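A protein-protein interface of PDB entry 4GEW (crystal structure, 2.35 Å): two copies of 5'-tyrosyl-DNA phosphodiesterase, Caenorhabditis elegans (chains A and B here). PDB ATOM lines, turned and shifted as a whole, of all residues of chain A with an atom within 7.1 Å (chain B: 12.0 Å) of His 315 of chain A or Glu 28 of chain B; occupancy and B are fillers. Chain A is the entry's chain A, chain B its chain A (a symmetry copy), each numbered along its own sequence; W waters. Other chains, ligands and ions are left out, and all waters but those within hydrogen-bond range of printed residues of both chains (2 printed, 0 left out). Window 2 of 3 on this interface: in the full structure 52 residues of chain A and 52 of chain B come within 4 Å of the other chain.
No position is printed for both chains.
Of the 6 pairs that touch across the chains among the printed residues, none has its exchanged pair printed and touching as well.
Among the printed residues, merely in contact across the chains: Arg 237 of chain A with Glu 26 of chain B, Arg 237 of chain A with Ile 29 of chain B, Gly 316 of chain A with Val 25 of chain B and Ala 317 of chain A with Val 25 of chain B.
Water W1 bridges the backbone carbonyl oxygen (O) of Gly 316 of chain A (2.8 Å) and the backbone carbonyl oxygen (O) of Glu 26 of chain B (2.9 Å).
Water W2 bridges N of Glu 28 of chain B (3.0 Å) and O of His 315 of chain A (3.2 Å).
N of Ala 317 of chain A lies within hydrogen-bond range of OG1 of Thr 305 of chain A (2.7 Å).
Of the printed residues of chain B, Arg 237 of chain A touches Glu 26, Ile 29 and Glu 32.
Thr 305 of chain A touches none of the printed residues of chain B.
Gln 312 of chain A touches none of the printed residues of chain B.
Phe 314 of chain A touches none of the printed residues of chain B.
His 315 of chain A touches just one residue of chain B: Glu 28.
Gly 316 of chain A touches just one residue of chain B: Val 25.
Ala 317 of chain A touches just one residue of chain B: Val 25.
Printed residues of chain A within 4 Å of Val 25 of chain B: Gly 316 and Ala 317.
Of chain A, only His 315 (2.3 Å) comes within 4 Å of Glu 28 of chain B.
Of the printed residues of chain A, Ile 29 of chain B touches Arg 237 (3.9 Å).
Leu 30 of chain B touches none of the printed residues of chain A.
Of the printed residues of chain A, Glu 32 of chain B touches Arg 237.
The nearest residue of chain B that does not touch His 315 of chain A is Glu 26 of chain B (6.4 Å).
Of the 14 printed residues of chain B, 5 touch a printed residue of chain A.
Hydrophobic or aromatic side chains of chain B within 4 Å of the printed part of chain A: Val 25 and Ile 29.
Of the 9 printed residues of chain A, 4 touch a printed residue of chain B.
Hydrophobic or aromatic side chains of chain A within 4 Å of the printed part of chain B: His 315 and Ala 317.
Among the printed residues, 6 pairs touch across the chains.
Among the printed residues, Asp or Glu carboxylates within 4 Å of a Lys or Arg side-chain nitrogen of the other chain: Arg 237 of chain A with Glu 32 of chain B (2.4 Å).
The side-chain carboxylate (OE1) of Glu 32 of chain B lies within salt-bridge range of the guanidinium group (NH1) of Arg 237 of chain A.
A ring nitrogen (ND1) of His 315 of chain A sits close to the side-chain carboxylate of Glu 28 of chain B (3.3 Å).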
ATOM      1  N   ARG A 237      19.892 -21.716  -5.995  1.00  0.00           N
ATOM      2  CA  ARG A 237      21.179 -21.296  -5.459  1.00  0.00           C
ATOM      3  C   ARG A 237      21.499 -19.844  -5.793  1.00  0.00           C
ATOM      4  O   ARG A 237      21.976 -19.093  -4.944  1.00  0.00           O
ATOM      5  CB  ARG A 237      22.299 -22.179  -6.007  1.00  0.00           C
ATOM      6  CG  ARG A 237      23.452 -22.336  -5.035  1.00  0.00           C
ATOM      7  CD  ARG A 237      24.661 -22.967  -5.685  1.00  0.00           C
ATOM      8  NE  ARG A 237      25.391 -22.002  -6.492  1.00  0.00           N
ATOM      9  CZ  ARG A 237      25.612 -22.123  -7.798  1.00  0.00           C
ATOM     10  NH1 ARG A 237      25.166 -23.183  -8.469  1.00  0.00           N
ATOM     11  NH2 ARG A 237      26.288 -21.178  -8.433  1.00  0.00           N
ATOM     12  N   THR A 305      16.532 -36.026  -4.564  1.00  0.00           N
ATOM     13  CA  THR A 305      16.222 -36.613  -5.866  1.00  0.00           C
ATOM     14  C   THR A 305      16.861 -37.987  -6.066  1.00  0.00           C
ATOM     15  O   THR A 305      16.565 -38.669  -7.049  1.00  0.00           O
ATOM     16  CB  THR A 305      16.631 -35.691  -7.037  1.00  0.00           C
ATOM     17  OG1 THR A 305      18.058 -35.566  -7.072  1.00  0.00           O
ATOM     18  CG2 THR A 305      15.995 -34.314  -6.882  1.00  0.00           C
ATOM     19  N   PHE A 306      17.745 -38.377  -5.150  1.00  0.00           N
ATOM     20  CA  PHE A 306      18.281 -39.740  -5.122  1.00  0.00           C
ATOM     21  C   PHE A 306      17.176 -40.716  -4.711  1.00  0.00           C
ATOM     22  O   PHE A 306      17.175 -41.876  -5.125  1.00  0.00           O
ATOM     23  CB  PHE A 306      19.424 -39.866  -4.105  1.00  0.00           C
ATOM     24  CG  PHE A 306      20.707 -39.194  -4.518  1.00  0.00           C
ATOM     25  CD1 PHE A 306      21.045 -37.949  -4.017  1.00  0.00           C
ATOM     26  CD2 PHE A 306      21.589 -39.824  -5.382  1.00  0.00           C
ATOM     27  CE1 PHE A 306      22.240 -37.337  -4.380  1.00  0.00           C
ATOM     28  CE2 PHE A 306      22.778 -39.215  -5.752  1.00  0.00           C
ATOM     29  CZ  PHE A 306      23.102 -37.970  -5.246  1.00  0.00           C
ATOM     30  N   GLN A 312      13.689 -35.319 -11.830  1.00  0.00           N
ATOM     31  CA  GLN A 312      14.844 -36.098 -12.255  1.00  0.00           C
ATOM     32  C   GLN A 312      15.910 -35.229 -12.908  1.00  0.00           C
ATOM     33  O   GLN A 312      15.630 -34.479 -13.844  1.00  0.00           O
ATOM     34  CB  GLN A 312      14.418 -37.188 -13.241  1.00  0.00           C
ATOM     35  CG  GLN A 312      13.334 -38.117 -12.728  1.00  0.00           C
ATOM     36  CD  GLN A 312      12.734 -38.961 -13.834  1.00  0.00           C
ATOM     37  OE1 GLN A 312      11.685 -38.625 -14.386  1.00  0.00           O
ATOM     38  NE2 GLN A 312      13.402 -40.059 -14.171  1.00  0.00           N
ATOM     39  N   GLY A 313      17.134 -35.343 -12.402  1.00  0.00           N
ATOM     40  CA  GLY A 313      18.294 -34.746 -13.034  1.00  0.00           C
ATOM     41  C   GLY A 313      19.219 -35.849 -13.507  1.00  0.00           C
ATOM     42  O   GLY A 313      19.002 -37.013 -13.186  1.00  0.00           O
ATOM     43  N   PHE A 314      20.236 -35.492 -14.288  1.00  0.00           N
ATOM     44  CA  PHE A 314      21.280 -36.435 -14.674  1.00  0.00           C
ATOM     45  C   PHE A 314      22.003 -36.925 -13.426  1.00  0.00           C
ATOM     46  O   PHE A 314      22.368 -38.090 -13.325  1.00  0.00           O
ATOM     47  CB  PHE A 314      22.275 -35.762 -15.624  1.00  0.00           C
ATOM     48  CG  PHE A 314      23.328 -36.690 -16.173  1.00  0.00           C
ATOM     49  CD1 PHE A 314      22.990 -37.699 -17.061  1.00  0.00           C
ATOM     50  CD2 PHE A 314      24.661 -36.534 -15.819  1.00  0.00           C
ATOM     51  CE1 PHE A 314      23.963 -38.549 -17.577  1.00  0.00           C
ATOM     52  CE2 PHE A 314      25.638 -37.379 -16.332  1.00  0.00           C
ATOM     53  CZ  PHE A 314      25.289 -38.387 -17.210  1.00  0.00           C
ATOM     54  N   HIS A 315      22.206 -36.019 -12.476  1.00  0.00           N
ATOM     55  CA  HIS A 315      22.843 -36.351 -11.211  1.00  0.00           C
ATOM     56  C   HIS A 315      21.885 -36.061 -10.067  1.00  0.00           C
ATOM     57  O   HIS A 315      21.153 -35.070 -10.096  1.00  0.00           O
ATOM     58  CB  HIS A 315      24.140 -35.555 -11.025  1.00  0.00           C
ATOM     59  CG  HIS A 315      25.257 -36.016 -11.909  1.00  0.00           C
ATOM     60  ND1 HIS A 315      26.302 -35.196 -12.280  1.00  0.00           N
ATOM     61  CD2 HIS A 315      25.486 -37.209 -12.504  1.00  0.00           C
ATOM     62  CE1 HIS A 315      27.126 -35.865 -13.067  1.00  0.00           C
ATOM     63  NE2 HIS A 315      26.654 -37.089 -13.220  1.00  0.00           N
ATOM     64  N   GLY A 316      21.886 -36.933  -9.064  1.00  0.00           N
ATOM     65  CA  GLY A 316      21.075 -36.718  -7.885  1.00  0.00           C
ATOM     66  C   GLY A 316      21.494 -35.459  -7.153  1.00  0.00           C
ATOM     67  O   GLY A 316      22.636 -35.006  -7.273  1.00  0.00           O
ATOM     68  N   ALA A 317      20.558 -34.886  -6.407  1.00  0.00           N
ATOM     69  CA  ALA A 317      20.824 -33.732  -5.565  1.00  0.00           C
ATOM     70  C   ALA A 317      20.045 -33.941  -4.277  1.00  0.00           C
ATOM     71  O   ALA A 317      19.035 -34.639  -4.285  1.00  0.00           O
ATOM     72  CB  ALA A 317      20.362 -32.469  -6.253  1.00  0.00           C
ATOM     73  N   SER B  23      26.814 -35.150   3.423  1.00  0.00           N
ATOM     74  CA  SER B  23      26.853 -33.754   3.030  1.00  0.00           C
ATOM     75  C   SER B  23      25.798 -33.522   1.961  1.00  0.00           C
ATOM     76  O   SER B  23      25.446 -34.439   1.217  1.00  0.00           O
ATOM     77  CB  SER B  23      28.233 -33.400   2.476  1.00  0.00           C
ATOM     78  OG  SER B  23      29.249 -33.678   3.425  1.00  0.00           O
ATOM     79  N   GLU B  24      25.290 -32.297   1.888  1.00  0.00           N
ATOM     80  CA  GLU B  24      24.309 -31.953   0.873  1.00  0.00           C
ATOM     81  C   GLU B  24      24.951 -32.035  -0.508  1.00  0.00           C
ATOM     82  O   GLU B  24      26.171 -31.924  -0.643  1.00  0.00           O
ATOM     83  CB  GLU B  24      23.719 -30.561   1.139  1.00  0.00           C
ATOM     84  CG  GLU B  24      24.730 -29.421   1.099  1.00  0.00           C
ATOM     85  CD  GLU B  24      24.197 -28.117   1.700  1.00  0.00           C
ATOM     86  OE1 GLU B  24      23.472 -28.161   2.722  1.00  0.00           O
ATOM     87  OE2 GLU B  24      24.516 -27.042   1.148  1.00  0.00           O
ATOM     88  N   VAL B  25      24.132 -32.265  -1.531  1.00  0.00           N
ATOM     89  CA  VAL B  25      24.612 -32.230  -2.903  1.00  0.00           C
ATOM     90  C   VAL B  25      23.845 -31.174  -3.688  1.00  0.00           C
ATOM     91  O   VAL B  25      22.616 -31.199  -3.741  1.00  0.00           O
ATOM     92  CB  VAL B  25      24.472 -33.592  -3.600  1.00  0.00           C
ATOM     93  CG1 VAL B  25      25.015 -33.510  -5.041  1.00  0.00           C
ATOM     94  CG2 VAL B  25      25.196 -34.668  -2.813  1.00  0.00           C
ATOM     95  N   GLU B  26      24.583 -30.253  -4.295  1.00  0.00           N
ATOM     96  CA  GLU B  26      24.008 -29.096  -4.969  1.00  0.00           C
ATOM     97  C   GLU B  26      23.475 -29.431  -6.364  1.00  0.00           C
ATOM     98  O   GLU B  26      24.023 -30.279  -7.070  1.00  0.00           O
ATOM     99  CB  GLU B  26      25.055 -27.975  -5.055  1.00  0.00           C
ATOM    100  CG  GLU B  26      24.541 -26.652  -5.609  1.00  0.00           C
ATOM    101  CD  GLU B  26      23.370 -26.093  -4.811  1.00  0.00           C
ATOM    102  OE1 GLU B  26      23.606 -25.469  -3.750  1.00  0.00           O
ATOM    103  OE2 GLU B  26      22.211 -26.277  -5.246  1.00  0.00           O
ATOM    104  N   ILE B  27      22.401 -28.748  -6.746  1.00  0.00           N
ATOM    105  CA  ILE B  27      21.788 -28.901  -8.057  1.00  0.00           C
ATOM    106  C   ILE B  27      22.739 -28.429  -9.152  1.00  0.00           C
ATOM    107  O   ILE B  27      23.307 -27.337  -9.063  1.00  0.00           O
ATOM    108  CB  ILE B  27      20.473 -28.087  -8.154  1.00  0.00           C
ATOM    109  CG1 ILE B  27      19.388 -28.685  -7.247  1.00  0.00           C
ATOM    110  CG2 ILE B  27      19.986 -27.999  -9.605  1.00  0.00           C
ATOM    111  CD1 ILE B  27      19.427 -28.189  -5.802  1.00  0.00           C
ATOM    112  N   GLU B  28      22.917 -29.254 -10.181  1.00  0.00           N
ATOM    113  CA  GLU B  28      23.730 -28.873 -11.332  1.00  0.00           C
ATOM    114  C   GLU B  28      23.003 -27.890 -12.233  1.00  0.00           C
ATOM    115  O   GLU B  28      21.831 -28.078 -12.550  1.00  0.00           O
ATOM    116  CB  GLU B  28      24.108 -30.100 -12.156  1.00  0.00           C
ATOM    117  CG  GLU B  28      25.127 -30.985 -11.491  1.00  0.00           C
ATOM    118  CD  GLU B  28      25.428 -32.219 -12.309  1.00  0.00           C
ATOM    119  OE1 GLU B  28      24.745 -32.435 -13.335  1.00  0.00           O
ATOM    120  OE2 GLU B  28      26.346 -32.972 -11.923  1.00  0.00           O
ATOM    121  N   ILE B  29      23.709 -26.847 -12.650  1.00  0.00           N
ATOM    122  CA  ILE B  29      23.190 -25.926 -13.655  1.00  0.00           C
ATOM    123  C   ILE B  29      24.067 -26.015 -14.902  1.00  0.00           C
ATOM    124  O   ILE B  29      25.238 -25.636 -14.889  1.00  0.00           O
ATOM    125  CB  ILE B  29      23.123 -24.487 -13.125  1.00  0.00           C
ATOM    126  CG1 ILE B  29      22.175 -24.423 -11.924  1.00  0.00           C
ATOM    127  CG2 ILE B  29      22.660 -23.538 -14.217  1.00  0.00           C
ATOM    128  CD1 ILE B  29      22.288 -23.155 -11.143  1.00  0.00           C
ATOM    129  N   LEU B  30      23.480 -26.522 -15.978  1.00  0.00           N
ATOM    130  CA  LEU B  30      24.229 -26.979 -17.138  1.00  0.00           C
ATOM    131  C   LEU B  30      25.039 -25.872 -17.827  1.00  0.00           C
ATOM    132  O   LEU B  30      26.153 -26.110 -18.295  1.00  0.00           O
ATOM    133  CB  LEU B  30      23.265 -27.657 -18.116  1.00  0.00           C
ATOM    134  CG  LEU B  30      23.763 -28.710 -19.104  1.00  0.00           C
ATOM    135  CD1 LEU B  30      24.461 -29.853 -18.394  1.00  0.00           C
ATOM    136  CD2 LEU B  30      22.587 -29.223 -19.916  1.00  0.00           C
ATOM    137  N   ASP B  31      24.493 -24.659 -17.876  1.00  0.00           N
ATOM    138  CA  ASP B  31      25.166 -23.558 -18.570  1.00  0.00           C
ATOM    139  C   ASP B  31      25.888 -22.592 -17.625  1.00  0.00           C
ATOM    140  O   ASP B  31      26.163 -21.447 -17.979  1.00  0.00           O
ATOM    141  CB  ASP B  31      24.183 -22.808 -19.474  1.00  0.00           C
ATOM    142  CG  ASP B  31      23.138 -22.041 -18.694  1.00  0.00           C
ATOM    143  OD1 ASP B  31      22.736 -22.502 -17.601  1.00  0.00           O
ATOM    144  OD2 ASP B  31      22.724 -20.968 -19.183  1.00  0.00           O
ATOM    145  N   GLU B  32      26.214 -23.077 -16.431  1.00  0.00           N
ATOM    146  CA  GLU B  32      26.956 -22.303 -15.439  1.00  0.00           C
ATOM    147  C   GLU B  32      28.456 -22.615 -15.520  1.00  0.00           C
ATOM    148  O   GLU B  32      28.828 -23.756 -15.776  1.00  0.00           O
ATOM    149  CB  GLU B  32      26.400 -22.634 -14.051  1.00  0.00           C
ATOM    150  CG  GLU B  32      27.313 -22.377 -12.876  1.00  0.00           C
ATOM    151  CD  GLU B  32      26.593 -22.529 -11.550  1.00  0.00           C
ATOM    152  OE1 GLU B  32      25.994 -23.601 -11.305  1.00  0.00           O
ATOM    153  OE2 GLU B  32      26.632 -21.574 -10.746  1.00  0.00           O
ATOM    154  N   PRO B  33      29.325 -21.601 -15.326  1.00  0.00           N
ATOM    155  CA  PRO B  33      30.781 -21.824 -15.326  1.00  0.00           C
ATOM    156  C   PRO B  33      31.139 -22.934 -14.342  1.00  0.00           C
ATOM    157  O   PRO B  33      30.693 -22.874 -13.201  1.00  0.00           O
ATOM    158  CB  PRO B  33      31.345 -20.489 -14.812  1.00  0.00           C
ATOM    159  CG  PRO B  33      30.308 -19.489 -15.142  1.00  0.00           C
ATOM    160  CD  PRO B  33      28.986 -20.199 -15.028  1.00  0.00           C
ATOM    161  N   GLU B  34      31.920 -23.920 -14.771  1.00  0.00           N
ATOM    162  CA  GLU B  34      32.087 -25.145 -13.992  1.00  0.00           C
ATOM    163  C   GLU B  34      33.256 -25.146 -13.014  1.00  0.00           C
ATOM    164  O   GLU B  34      33.900 -26.176 -12.802  1.00  0.00           O
ATOM    165  CB  GLU B  34      32.157 -26.378 -14.903  1.00  0.00           C
ATOM    166  CG  GLU B  34      33.329 -26.399 -15.860  1.00  0.00           C
ATOM    167  CD  GLU B  34      32.971 -25.866 -17.230  1.00  0.00           C
ATOM    168  OE1 GLU B  34      32.852 -24.632 -17.375  1.00  0.00           O
ATOM    169  OE2 GLU B  34      32.806 -26.683 -18.160  1.00  0.00           O
ATOM    170  N   GLN B  35      33.517 -24.001 -12.403  1.00  0.00           N
ATOM    171  CA  GLN B  35      34.507 -23.926 -11.337  1.00  0.00           C
ATOM    172  C   GLN B  35      34.145 -22.842 -10.339  1.00  0.00           C
ATOM    173  O   GLN B  35      33.940 -21.686 -10.714  1.00  0.00           O
ATOM    174  CB  GLN B  35      35.915 -23.672 -11.893  1.00  0.00           C
ATOM    175  CG  GLN B  35      36.729 -24.935 -12.169  1.00  0.00           C
ATOM    176  CD  GLN B  35      38.196 -24.641 -12.454  1.00  0.00           C
ATOM    177  OE1 GLN B  35      38.740 -23.628 -12.009  1.00  0.00           O
ATOM    178  NE2 GLN B  35      38.842 -25.533 -13.196  1.00  0.00           N
ATOM    179  N   GLY B  36      34.047 -23.220  -9.071  1.00  0.00           N
ATOM    180  CA  GLY B  36      33.908 -22.241  -8.014  1.00  0.00           C
ATOM    181  C   GLY B  36      35.207 -21.472  -7.915  1.00  0.00           C
ATOM    182  O   GLY B  36      36.288 -22.060  -7.952  1.00  0.00           O
HETATM  183  O   HOH W   1      23.317 -32.626  -8.557  1.00  0.00           O
HETATM  184  O   HOH W   2      21.504 -31.849 -10.153  1.00  0.00           O
